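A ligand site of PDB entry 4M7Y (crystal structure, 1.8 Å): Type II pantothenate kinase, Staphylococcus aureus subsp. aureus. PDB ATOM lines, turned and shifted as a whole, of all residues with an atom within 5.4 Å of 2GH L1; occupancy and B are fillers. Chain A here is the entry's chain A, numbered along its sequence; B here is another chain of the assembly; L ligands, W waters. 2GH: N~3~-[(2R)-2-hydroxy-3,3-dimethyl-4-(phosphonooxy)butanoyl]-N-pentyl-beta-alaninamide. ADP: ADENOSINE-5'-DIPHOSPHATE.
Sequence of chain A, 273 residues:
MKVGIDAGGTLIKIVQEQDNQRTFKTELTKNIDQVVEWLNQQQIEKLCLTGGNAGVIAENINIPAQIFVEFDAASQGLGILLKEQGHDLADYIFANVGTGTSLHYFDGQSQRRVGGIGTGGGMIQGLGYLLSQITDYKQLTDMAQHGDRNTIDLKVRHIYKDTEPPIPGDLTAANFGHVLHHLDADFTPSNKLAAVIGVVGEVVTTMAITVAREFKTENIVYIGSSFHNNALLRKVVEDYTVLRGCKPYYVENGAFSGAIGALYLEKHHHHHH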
ATOM      1  N   GLY A   8      34.773  11.487  23.327  1.00  0.00           N
ATOM      2  CA  GLY A   8      34.422  12.691  22.561  1.00  0.00           C
ATOM      3  C   GLY A   8      35.498  13.748  22.624  1.00  0.00           C
ATOM      4  O   GLY A   8      36.626  13.486  23.050  1.00  0.00           O
ATOM      5  N   GLY A   9      35.128  14.974  22.219  1.00  0.00           N
ATOM      6  CA  GLY A   9      36.034  16.089  22.202  1.00  0.00           C
ATOM      7  C   GLY A   9      36.363  16.620  23.594  1.00  0.00           C
ATOM      8  O   GLY A   9      37.381  17.225  23.753  1.00  0.00           O
ATOM      9  N   GLU A  70      29.238   7.256  15.872  1.00  0.00           N
ATOM     10  CA  GLU A  70      28.585   7.789  17.057  1.00  0.00           C
ATOM     11  C   GLU A  70      27.112   8.149  16.869  1.00  0.00           C
ATOM     12  O   GLU A  70      26.339   8.079  17.819  1.00  0.00           O
ATOM     13  CB  GLU A  70      29.394   8.941  17.662  1.00  0.00           C
ATOM     14  CG  GLU A  70      29.274  10.281  16.972  1.00  0.00           C
ATOM     15  CD  GLU A  70      29.884  11.381  17.815  1.00  0.00           C
ATOM     16  OE1 GLU A  70      29.193  11.895  18.739  1.00  0.00           O
ATOM     17  OE2 GLU A  70      31.038  11.705  17.592  1.00  0.00           O
ATOM     18  N   PHE A  71      26.727   8.523  15.639  1.00  0.00           N
ATOM     19  CA  PHE A  71      25.346   8.867  15.373  1.00  0.00           C
ATOM     20  C   PHE A  71      24.419   7.645  15.587  1.00  0.00           C
ATOM     21  O   PHE A  71      23.433   7.741  16.310  1.00  0.00           O
ATOM     22  CB  PHE A  71      25.196   9.464  13.967  1.00  0.00           C
ATOM     23  CG  PHE A  71      26.075  10.701  13.731  1.00  0.00           C
ATOM     24  CD1 PHE A  71      26.394  11.587  14.763  1.00  0.00           C
ATOM     25  CD2 PHE A  71      26.548  10.984  12.459  1.00  0.00           C
ATOM     26  CE1 PHE A  71      27.180  12.715  14.527  1.00  0.00           C
ATOM     27  CE2 PHE A  71      27.334  12.112  12.222  1.00  0.00           C
ATOM     28  CZ  PHE A  71      27.649  12.967  13.257  1.00  0.00           C
ATOM     29  N   ASN A  96      21.815  16.146  20.436  1.00  0.00           N
ATOM     30  CA  ASN A  96      22.995  15.743  21.167  1.00  0.00           C
ATOM     31  C   ASN A  96      23.898  16.953  21.400  1.00  0.00           C
ATOM     32  O   ASN A  96      24.660  17.381  20.515  1.00  0.00           O
ATOM     33  CB  ASN A  96      23.724  14.637  20.403  1.00  0.00           C
ATOM     34  CG  ASN A  96      24.725  13.890  21.260  1.00  0.00           C
ATOM     35  OD1 ASN A  96      25.148  14.361  22.329  1.00  0.00           O
ATOM     36  ND2 ASN A  96      25.094  12.698  20.821  1.00  0.00           N
ATOM     37  N   GLY A  98      26.800  18.035  22.854  1.00  0.00           N
ATOM     38  CA  GLY A  98      28.157  17.665  23.313  1.00  0.00           C
ATOM     39  C   GLY A  98      29.112  18.831  23.236  1.00  0.00           C
ATOM     40  O   GLY A  98      28.716  19.974  23.444  1.00  0.00           O
ATOM     41  N   THR A  99      30.365  18.590  22.874  1.00  0.00           N
ATOM     42  CA  THR A  99      31.256  19.707  22.687  1.00  0.00           C
ATOM     43  C   THR A  99      30.561  20.669  21.696  1.00  0.00           C
ATOM     44  O   THR A  99      30.626  21.902  21.847  1.00  0.00           O
ATOM     45  CB  THR A  99      32.629  19.233  22.231  1.00  0.00           C
ATOM     46  OG1 THR A  99      33.184  18.402  23.258  1.00  0.00           O
ATOM     47  CG2 THR A  99      33.558  20.411  21.956  1.00  0.00           C
ATOM     48  N   GLY A 100      29.888  20.075  20.713  1.00  0.00           N
ATOM     49  CA  GLY A 100      29.027  20.800  19.799  1.00  0.00           C
ATOM     50  C   GLY A 100      27.719  20.051  19.664  1.00  0.00           C
ATOM     51  O   GLY A 100      27.522  19.022  20.295  1.00  0.00           O
ATOM     52  N   THR A 101      26.856  20.537  18.778  1.00  0.00           N
ATOM     53  CA  THR A 101      25.477  20.065  18.734  1.00  0.00           C
ATOM     54  C   THR A 101      25.131  19.408  17.405  1.00  0.00           C
ATOM     55  O   THR A 101      25.341  19.976  16.303  1.00  0.00           O
ATOM     56  CB  THR A 101      24.515  21.190  19.137  1.00  0.00           C
ATOM     57  OG1 THR A 101      24.842  21.645  20.442  1.00  0.00           O
ATOM     58  CG2 THR A 101      23.058  20.720  19.143  1.00  0.00           C
ATOM     59  N   SER A 102      24.677  18.150  17.512  1.00  0.00           N
ATOM     60  CA  SER A 102      24.249  17.355  16.397  1.00  0.00           C
ATOM     61  C   SER A 102      22.764  16.998  16.553  1.00  0.00           C
ATOM     62  O   SER A 102      22.328  16.560  17.649  1.00  0.00           O
ATOM     63  CB  SER A 102      25.113  16.079  16.335  1.00  0.00           C
ATOM     64  OG  SER A 102      24.958  15.414  15.098  1.00  0.00           O
ATOM     65  N   ARG A 113      20.810  12.244  10.481  1.00  0.00           N
ATOM     66  CA  ARG A 113      21.228  13.569  10.936  1.00  0.00           C
ATOM     67  C   ARG A 113      20.479  14.609  10.118  1.00  0.00           C
ATOM     68  O   ARG A 113      20.409  14.499   8.906  1.00  0.00           O
ATOM     69  CB  ARG A 113      22.726  13.743  10.798  1.00  0.00           C
ATOM     70  CG  ARG A 113      23.271  14.945  11.515  1.00  0.00           C
ATOM     71  CD  ARG A 113      24.774  14.880  11.623  1.00  0.00           C
ATOM     72  NE  ARG A 113      25.349  15.981  12.402  1.00  0.00           N
ATOM     73  CZ  ARG A 113      25.631  17.180  11.923  1.00  0.00           C
ATOM     74  NH1 ARG A 113      25.377  17.464  10.641  1.00  0.00           N
ATOM     75  NH2 ARG A 113      26.183  18.102  12.698  1.00  0.00           N
ATOM     76  N   GLY A 115      20.627  18.173  11.174  1.00  0.00           N
ATOM     77  CA  GLY A 115      21.083  19.462  11.617  1.00  0.00           C
ATOM     78  C   GLY A 115      22.304  19.377  12.529  1.00  0.00           C
ATOM     79  O   GLY A 115      22.590  18.333  13.116  1.00  0.00           O
ATOM     80  N   GLY A 116      23.031  20.489  12.605  1.00  0.00           N
ATOM     81  CA  GLY A 116      24.063  20.655  13.596  1.00  0.00           C
ATOM     82  C   GLY A 116      24.434  22.111  13.754  1.00  0.00           C
ATOM     83  O   GLY A 116      24.162  22.925  12.882  1.00  0.00           O
ATOM     84  N   ILE A 117      25.142  22.414  14.838  1.00  0.00           N
ATOM     85  CA  ILE A 117      25.530  23.783  15.114  1.00  0.00           C
ATOM     86  C   ILE A 117      26.636  23.803  16.191  1.00  0.00           C
ATOM     87  O   ILE A 117      26.701  22.924  17.053  1.00  0.00           O
ATOM     88  CB  ILE A 117      24.271  24.642  15.499  1.00  0.00           C
ATOM     89  CG1 ILE A 117      24.564  26.152  15.541  1.00  0.00           C
ATOM     90  CG2 ILE A 117      23.617  24.172  16.782  1.00  0.00           C
ATOM     91  CD1 ILE A 117      24.974  26.720  14.183  1.00  0.00           C
ATOM     92  N   GLY A 118      27.539  24.782  16.096  1.00  0.00           N
ATOM     93  CA  GLY A 118      28.654  24.925  17.045  1.00  0.00           C
ATOM     94  C   GLY A 118      28.307  25.520  18.409  1.00  0.00           C
ATOM     95  O   GLY A 118      29.186  25.717  19.244  1.00  0.00           O
ATOM     96  N   VAL B 156      35.359  20.020  13.483  1.00  0.00           N
ATOM     97  CA  VAL B 156      35.111  18.577  13.486  1.00  0.00           C
ATOM     98  C   VAL B 156      36.440  17.768  13.431  1.00  0.00           C
ATOM     99  O   VAL B 156      36.604  16.778  14.158  1.00  0.00           O
ATOM    100  CB  VAL B 156      34.184  18.175  12.302  1.00  0.00           C
ATOM    101  CG1 VAL B 156      34.053  16.651  12.196  1.00  0.00           C
ATOM    102  CG2 VAL B 156      32.829  18.842  12.443  1.00  0.00           C
ATOM    103  N   ILE B 159      38.089  17.160  16.806  1.00  0.00           N
ATOM    104  CA  ILE B 159      37.401  16.133  17.631  1.00  0.00           C
ATOM    105  C   ILE B 159      37.743  14.738  17.118  1.00  0.00           C
ATOM    106  O   ILE B 159      38.196  13.885  17.892  1.00  0.00           O
ATOM    107  CB  ILE B 159      35.874  16.402  17.674  1.00  0.00           C
ATOM    108  CG1 ILE B 159      35.635  17.773  18.350  1.00  0.00           C
ATOM    109  CG2 ILE B 159      35.103  15.290  18.420  1.00  0.00           C
ATOM    110  CD1 ILE B 159      34.192  18.089  18.709  1.00  0.00           C
ATOM    111  N   TYR B 160      37.552  14.507  15.808  1.00  0.00           N
ATOM    112  CA  TYR B 160      38.005  13.251  15.152  1.00  0.00           C
ATOM    113  C   TYR B 160      39.515  13.234  14.862  1.00  0.00           C
ATOM    114  O   TYR B 160      39.960  13.466  13.727  1.00  0.00           O
ATOM    115  CB  TYR B 160      37.158  12.966  13.884  1.00  0.00           C
ATOM    116  CG  TYR B 160      35.830  12.400  14.277  1.00  0.00           C
ATOM    117  CD1 TYR B 160      34.816  13.225  14.782  1.00  0.00           C
ATOM    118  CD2 TYR B 160      35.604  11.024  14.248  1.00  0.00           C
ATOM    119  CE1 TYR B 160      33.609  12.716  15.185  1.00  0.00           C
ATOM    120  CE2 TYR B 160      34.394  10.485  14.652  1.00  0.00           C
ATOM    121  CZ  TYR B 160      33.395  11.315  15.115  1.00  0.00           C
ATOM    122  OH  TYR B 160      32.198  10.775  15.534  1.00  0.00           O
ATOM    123  N   ILE B 167      31.183  13.686   9.288  1.00  0.00           N
ATOM    124  CA  ILE B 167      30.724  14.823   8.527  1.00  0.00           C
ATOM    125  C   ILE B 167      31.964  15.655   8.184  1.00  0.00           C
ATOM    126  O   ILE B 167      33.018  15.430   8.757  1.00  0.00           O
ATOM    127  CB  ILE B 167      29.702  15.645   9.323  1.00  0.00           C
ATOM    128  CG1 ILE B 167      30.357  16.325  10.528  1.00  0.00           C
ATOM    129  CG2 ILE B 167      28.554  14.757   9.782  1.00  0.00           C
ATOM    130  CD1 ILE B 167      29.431  17.282  11.252  1.00  0.00           C
ATOM    131  N   LEU B 171      34.144  21.834   9.027  1.00  0.00           N
ATOM    132  CA  LEU B 171      33.036  22.537   9.660  1.00  0.00           C
ATOM    133  C   LEU B 171      33.398  22.883  11.077  1.00  0.00           C
ATOM    134  O   LEU B 171      34.136  22.137  11.716  1.00  0.00           O
ATOM    135  CB  LEU B 171      31.749  21.673   9.680  1.00  0.00           C
ATOM    136  CG  LEU B 171      31.139  21.291   8.323  1.00  0.00           C
ATOM    137  CD1 LEU B 171      30.149  20.135   8.492  1.00  0.00           C
ATOM    138  CD2 LEU B 171      30.458  22.483   7.673  1.00  0.00           C
ATOM    139  N   THR B 172      32.859  24.018  11.555  1.00  0.00           N
ATOM    140  CA  THR B 172      32.937  24.370  12.959  1.00  0.00           C
ATOM    141  C   THR B 172      32.123  23.368  13.769  1.00  0.00           C
ATOM    142  O   THR B 172      30.951  23.171  13.510  1.00  0.00           O
ATOM    143  CB  THR B 172      32.359  25.761  13.225  1.00  0.00           C
ATOM    144  OG1 THR B 172      33.024  26.710  12.390  1.00  0.00           O
ATOM    145  CG2 THR B 172      32.586  26.156  14.668  1.00  0.00           C
ATOM    146  N   ALA B 173      32.768  22.734  14.736  1.00  0.00           N
ATOM    147  CA  ALA B 173      32.120  21.806  15.612  1.00  0.00           C
ATOM    148  C   ALA B 173      31.596  22.518  16.864  1.00  0.00           C
ATOM    149  O   ALA B 173      30.463  22.247  17.353  1.00  0.00           O
ATOM    150  CB  ALA B 173      33.096  20.692  15.987  1.00  0.00           C
ATOM    151  N   ALA B 174      32.406  23.443  17.382  1.00  0.00           N
ATOM    152  CA  ALA B 174      32.087  24.198  18.589  1.00  0.00           C
ATOM    153  C   ALA B 174      32.701  25.596  18.459  1.00  0.00           C
ATOM    154  O   ALA B 174      33.931  25.735  18.345  1.00  0.00           O
ATOM    155  CB  ALA B 174      32.651  23.497  19.800  1.00  0.00           C
ATOM    156  N   GLU B 202      27.242  31.931  11.447  1.00  0.00           N
ATOM    157  CA  GLU B 202      26.942  30.479  11.330  1.00  0.00           C
ATOM    158  C   GLU B 202      25.569  30.118  11.854  1.00  0.00           C
ATOM    159  O   GLU B 202      24.878  29.275  11.252  1.00  0.00           O
ATOM    160  CB  GLU B 202      27.991  29.658  12.064  1.00  0.00           C
ATOM    161  CG  GLU B 202      29.349  29.732  11.436  1.00  0.00           C
ATOM    162  CD  GLU B 202      30.400  28.932  12.183  1.00  0.00           C
ATOM    163  OE1 GLU B 202      30.078  28.323  13.195  1.00  0.00           O
ATOM    164  OE2 GLU B 202      31.555  28.932  11.751  1.00  0.00           O
ATOM    165  N   THR B 206      22.835  28.611   9.339  1.00  0.00           N
ATOM    166  CA  THR B 206      22.374  27.241   9.601  1.00  0.00           C
ATOM    167  C   THR B 206      20.851  27.201   9.718  1.00  0.00           C
ATOM    168  O   THR B 206      20.201  26.295   9.198  1.00  0.00           O
ATOM    169  CB  THR B 206      23.097  26.663  10.847  1.00  0.00           C
ATOM    170  OG1 THR B 206      24.516  26.607  10.573  1.00  0.00           O
ATOM    171  CG2 THR B 206      22.610  25.259  11.161  1.00  0.00           C
ATOM    172  N   TYR B 240      28.894  29.373   3.803  1.00  0.00           N
ATOM    173  CA  TYR B 240      28.147  28.227   4.352  1.00  0.00           C
ATOM    174  C   TYR B 240      26.815  28.003   3.614  1.00  0.00           C
ATOM    175  O   TYR B 240      26.371  26.872   3.495  1.00  0.00           O
ATOM    176  CB  TYR B 240      27.952  28.338   5.884  1.00  0.00           C
ATOM    177  CG  TYR B 240      27.441  27.023   6.469  1.00  0.00           C
ATOM    178  CD1 TYR B 240      28.167  25.841   6.311  1.00  0.00           C
ATOM    179  CD2 TYR B 240      26.226  26.953   7.138  1.00  0.00           C
ATOM    180  CE1 TYR B 240      27.698  24.637   6.819  1.00  0.00           C
ATOM    181  CE2 TYR B 240      25.751  25.751   7.653  1.00  0.00           C
ATOM    182  CZ  TYR B 240      26.487  24.597   7.486  1.00  0.00           C
ATOM    183  OH  TYR B 240      26.013  23.404   8.001  1.00  0.00           O
HETATM  184  OAH 2GH L   1      29.307  15.369  20.827  1.00  0.00           O
HETATM  185  PAX 2GH L   1      30.518  15.913  19.955  1.00  0.00           P
HETATM  186  OAI 2GH L   1      31.901  15.194  20.390  1.00  0.00           O
HETATM  187  OAF 2GH L   1      30.680  17.397  19.957  1.00  0.00           O
HETATM  188  OAS 2GH L   1      30.254  15.339  18.479  1.00  0.00           O
HETATM  189  CAP 2GH L   1      31.098  15.789  17.444  1.00  0.00           C
HETATM  190  CAW 2GH L   1      30.266  16.460  16.342  1.00  0.00           C
HETATM  191  CAB 2GH L   1      29.302  15.381  15.784  1.00  0.00           C
HETATM  192  CAC 2GH L   1      31.232  16.981  15.246  1.00  0.00           C
HETATM  193  CAV 2GH L   1      29.421  17.664  16.975  1.00  0.00           C
HETATM  194  OAG 2GH L   1      30.324  18.547  17.679  1.00  0.00           O
HETATM  195  CAU 2GH L   1      28.653  18.448  15.887  1.00  0.00           C
HETATM  196  OAE 2GH L   1      27.827  17.887  15.144  1.00  0.00           O
HETATM  197  NAR 2GH L   1      28.936  19.763  15.842  1.00  0.00           N
HETATM  198  CAN 2GH L   1      28.269  20.673  14.889  1.00  0.00           C
HETATM  199  CAO 2GH L   1      28.936  20.520  13.505  1.00  0.00           C
HETATM  200  CAT 2GH L   1      28.048  21.202  12.460  1.00  0.00           C
HETATM  201  OAD 2GH L   1      27.050  20.639  12.029  1.00  0.00           O
HETATM  202  NAQ 2GH L   1      28.385  22.432  12.128  1.00  0.00           N
HETATM  203  CAM 2GH L   1      27.558  23.200  11.141  1.00  0.00           C
HETATM  204  CAL 2GH L   1      27.684  24.692  11.391  1.00  0.00           C
HETATM  205  CAK 2GH L   1      29.049  25.156  10.897  1.00  0.00           C
HETATM  206  CAJ 2GH L   1      28.942  26.371   9.988  1.00  0.00           C
HETATM  207  CAA 2GH L   1      30.195  26.513   9.074  1.00  0.00           C
HETATM  208  PB  ADP L   2      31.926  15.095  23.908  1.00  0.00           P
HETATM  209  O1B ADP L   2      32.265  15.945  22.726  1.00  0.00           O
HETATM  210  O2B ADP L   2      31.425  13.741  23.462  1.00  0.00           O
HETATM  211  O3B ADP L   2      33.004  15.065  24.938  1.00  0.00           O
HETATM  212  PA  ADP L   2      29.700  15.661  25.858  1.00  0.00           P
HETATM  213  O1A ADP L   2      30.379  14.856  26.919  1.00  0.00           O
HETATM  214  O2A ADP L   2      28.336  15.194  25.389  1.00  0.00           O
HETATM  215  O3A ADP L   2      30.685  15.937  24.556  1.00  0.00           O
HETATM  216  O5' ADP L   2      29.626  17.152  26.350  1.00  0.00           O
HETATM  217  C5' ADP L   2      30.814  17.918  26.691  1.00  0.00           C
HETATM  218  C4' ADP L   2      30.345  19.159  27.418  1.00  0.00           C
HETATM  219  O4' ADP L   2      29.698  18.797  28.659  1.00  0.00           O
HETATM  220  C3' ADP L   2      31.448  20.097  27.756  1.00  0.00           C
HETATM  221  O3' ADP L   2      31.793  20.992  26.671  1.00  0.00           O
HETATM  222  C2' ADP L   2      30.903  20.809  28.945  1.00  0.00           C
HETATM  223  O2' ADP L   2      30.079  21.883  28.558  1.00  0.00           O
HETATM  224  C1' ADP L   2      30.032  19.748  29.639  1.00  0.00           C
HETATM  225  N9  ADP L   2      30.623  19.092  30.812  1.00  0.00           N
HETATM  226  C8  ADP L   2      29.886  18.357  31.693  1.00  0.00           C
HETATM  227  N7  ADP L   2      30.629  17.873  32.685  1.00  0.00           N
HETATM  228  C5  ADP L   2      31.879  18.286  32.471  1.00  0.00           C
HETATM  229  C6  ADP L   2      33.124  18.105  33.154  1.00  0.00           C
HETATM  230  N6  ADP L   2      33.156  17.368  34.314  1.00  0.00           N
HETATM  231  N1  ADP L   2      34.249  18.700  32.655  1.00  0.00           N
HETATM  232  C2  ADP L   2      34.220  19.407  31.518  1.00  0.00           C
HETATM  233  N3  ADP L   2      33.062  19.597  30.820  1.00  0.00           N
HETATM  234  C4  ADP L   2      31.897  19.073  31.238  1.00  0.00           C
HETATM  235  O   HOH W   1      27.019  15.862  19.524  1.00  0.00           O
HETATM  236  O   HOH W   2      32.739  12.759  19.196  1.00  0.00           O
HETATM  237  O   HOH W   3      28.033  14.131  22.843  1.00  0.00           O
HETATM  238  O   HOH W   4      25.357  20.361   9.865  1.00  0.00           O
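The backbone carbonyl oxygen (O) of Thr 101 lies close to an oxygen (OAE) of 2GH L1 (3.4 Å). Gly 9 touches 2GH L1. OE1 of Glu 70 touches OAS of 2GH L1, 3.6 Å away. Phe 71 touches 2GH L1 (CE1 to CAB, 3.6 Å). CA of Gly 98 touches OAH of 2GH L1, at 3.6 Å. Ser 102 touches 2GH L1. Gly 116 touches 2GH L1 (CA to OAD, 3.4 Å). Ile 117 touches 2GH L1. CG2 of Val 156 of chain B touches CAC of 2GH L1, at 3.7 Å. Ile 159 of chain B touches 2GH L1 (CG2 to OAI, 3.8 Å). Ile 167 of chain B touches 2GH L1. Glu 202 of chain B touches 2GH L1 (CD to CAJ, 3.7 Å). Thr 206 of chain B touches 2GH L1 (OG1 to CAL, 3.8 Å). Tyr 240 of chain B touches 2GH L1. Hydrophobic or aromatic side chains within 4 Å of 2GH L1: Phe 71, Val 156 of chain B, Ile 159 of chain B, Ile 167 of chain B, Ala 173 of chain B and Tyr 240 of chain B. 19 residues have an atom within 4 Å of 2GH L1: Gly 9, Glu 70, Phe 71, Gly 98, Thr 99, Gly 100, Thr 101, Ser 102, Arg 113, Gly 116, Ile 117, Val 156 of chain B, Ile 159 of chain B, Ile 167 of chain B, Thr 172 of chain B, Ala 173 of chain B, Glu 202 of chain B, Thr 206 of chain B and Tyr 240 of chain B. Along chain A the residues within 4 Å of 2GH L1 span positions 9 to 117. The nearest printed residue that does not touch 2GH L1 is Gly 8 (4.2 Å).
An oxygen (O1B) of ADP L2 sits at hydrogen-bond distance from the backbone NH of Gly 9 (3.1 Å). A nitrogen (NAR) of 2GH L1 sits at hydrogen-bond distance from the backbone carbonyl oxygen of Ala 173 of chain B (3.3 Å). NH2 of Arg 113 lies within hydrogen-bond range of OAD of 2GH L1 (2.8 Å). The side-chain hydroxyl of Thr 99 sits at hydrogen-bond distance from an oxygen (O1B) of ADP L2 (2.7 Å). An oxygen (OAF) of 2GH L1 sits at hydrogen-bond distance from the backbone NH (N) of Gly 100. NAQ of 2GH L1 lies within hydrogen-bond range of O of Thr 172 of chain B (3.0 Å). N of Thr 99 sits at hydrogen-bond distance from O3A of ADP L2 (3.2 Å). N of Thr 99 is in hydrogen-bond range of OAF of 2GH L1 (3.2 Å).
OE2 of Glu 202 of chain B sits at hydrogen-bond distance from OG1 of Thr 172 of chain B (2.7 Å). The backbone carbonyl oxygen of Thr 101 is in hydrogen-bond range of the backbone NH of Ile 117 (2.9 Å). OE2 of Glu 70 sits at hydrogen-bond distance from OH of Tyr 160 of chain B (2.5 Å). The guanidinium group (NE) of Arg 113 lies within hydrogen-bond range of the side-chain hydroxyl (OG) of Ser 102 (2.8 Å). The side-chain hydroxyl of Thr 206 of chain B lies within hydrogen-bond range of the backbone carbonyl oxygen of Glu 202 of chain B, at 2.8 Å. O of Ser 102 sits at hydrogen-bond distance from N of Asn 96, 2.9 Å away. The backbone NH (N) of Val 156 of chain B lies within hydrogen-bond range of the backbone carbonyl oxygen (O) of Leu 171 of chain B, 3.0 Å away.
An oxygen (OAI) of 2GH L1 sits close to an oxygen (O1B) of ADP L2, 2.5 Å away.
Water W1 lies within hydrogen-bond range of OAH of 2GH L1 (2.7 Å), O of Asn 96 (3.0 Å) and O of Gly 100 (3.3 Å). Water W3 lies within hydrogen-bond range of an oxygen (OAH) of 2GH L1, an oxygen (O2A) of ADP L2 and the side-chain amide oxygen (OD1) of Asn 96. Water W4 bridges an oxygen (OAD) of 2GH L1 (2.8 Å) and the guanidinium group (NH1) of Arg 113 (3.0 Å). Water W2 lies within hydrogen-bond range of the side-chain carboxylate (OE2) of Glu 70 (2.6 Å) and an oxygen (OAI) of 2GH L1 (2.8 Å).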
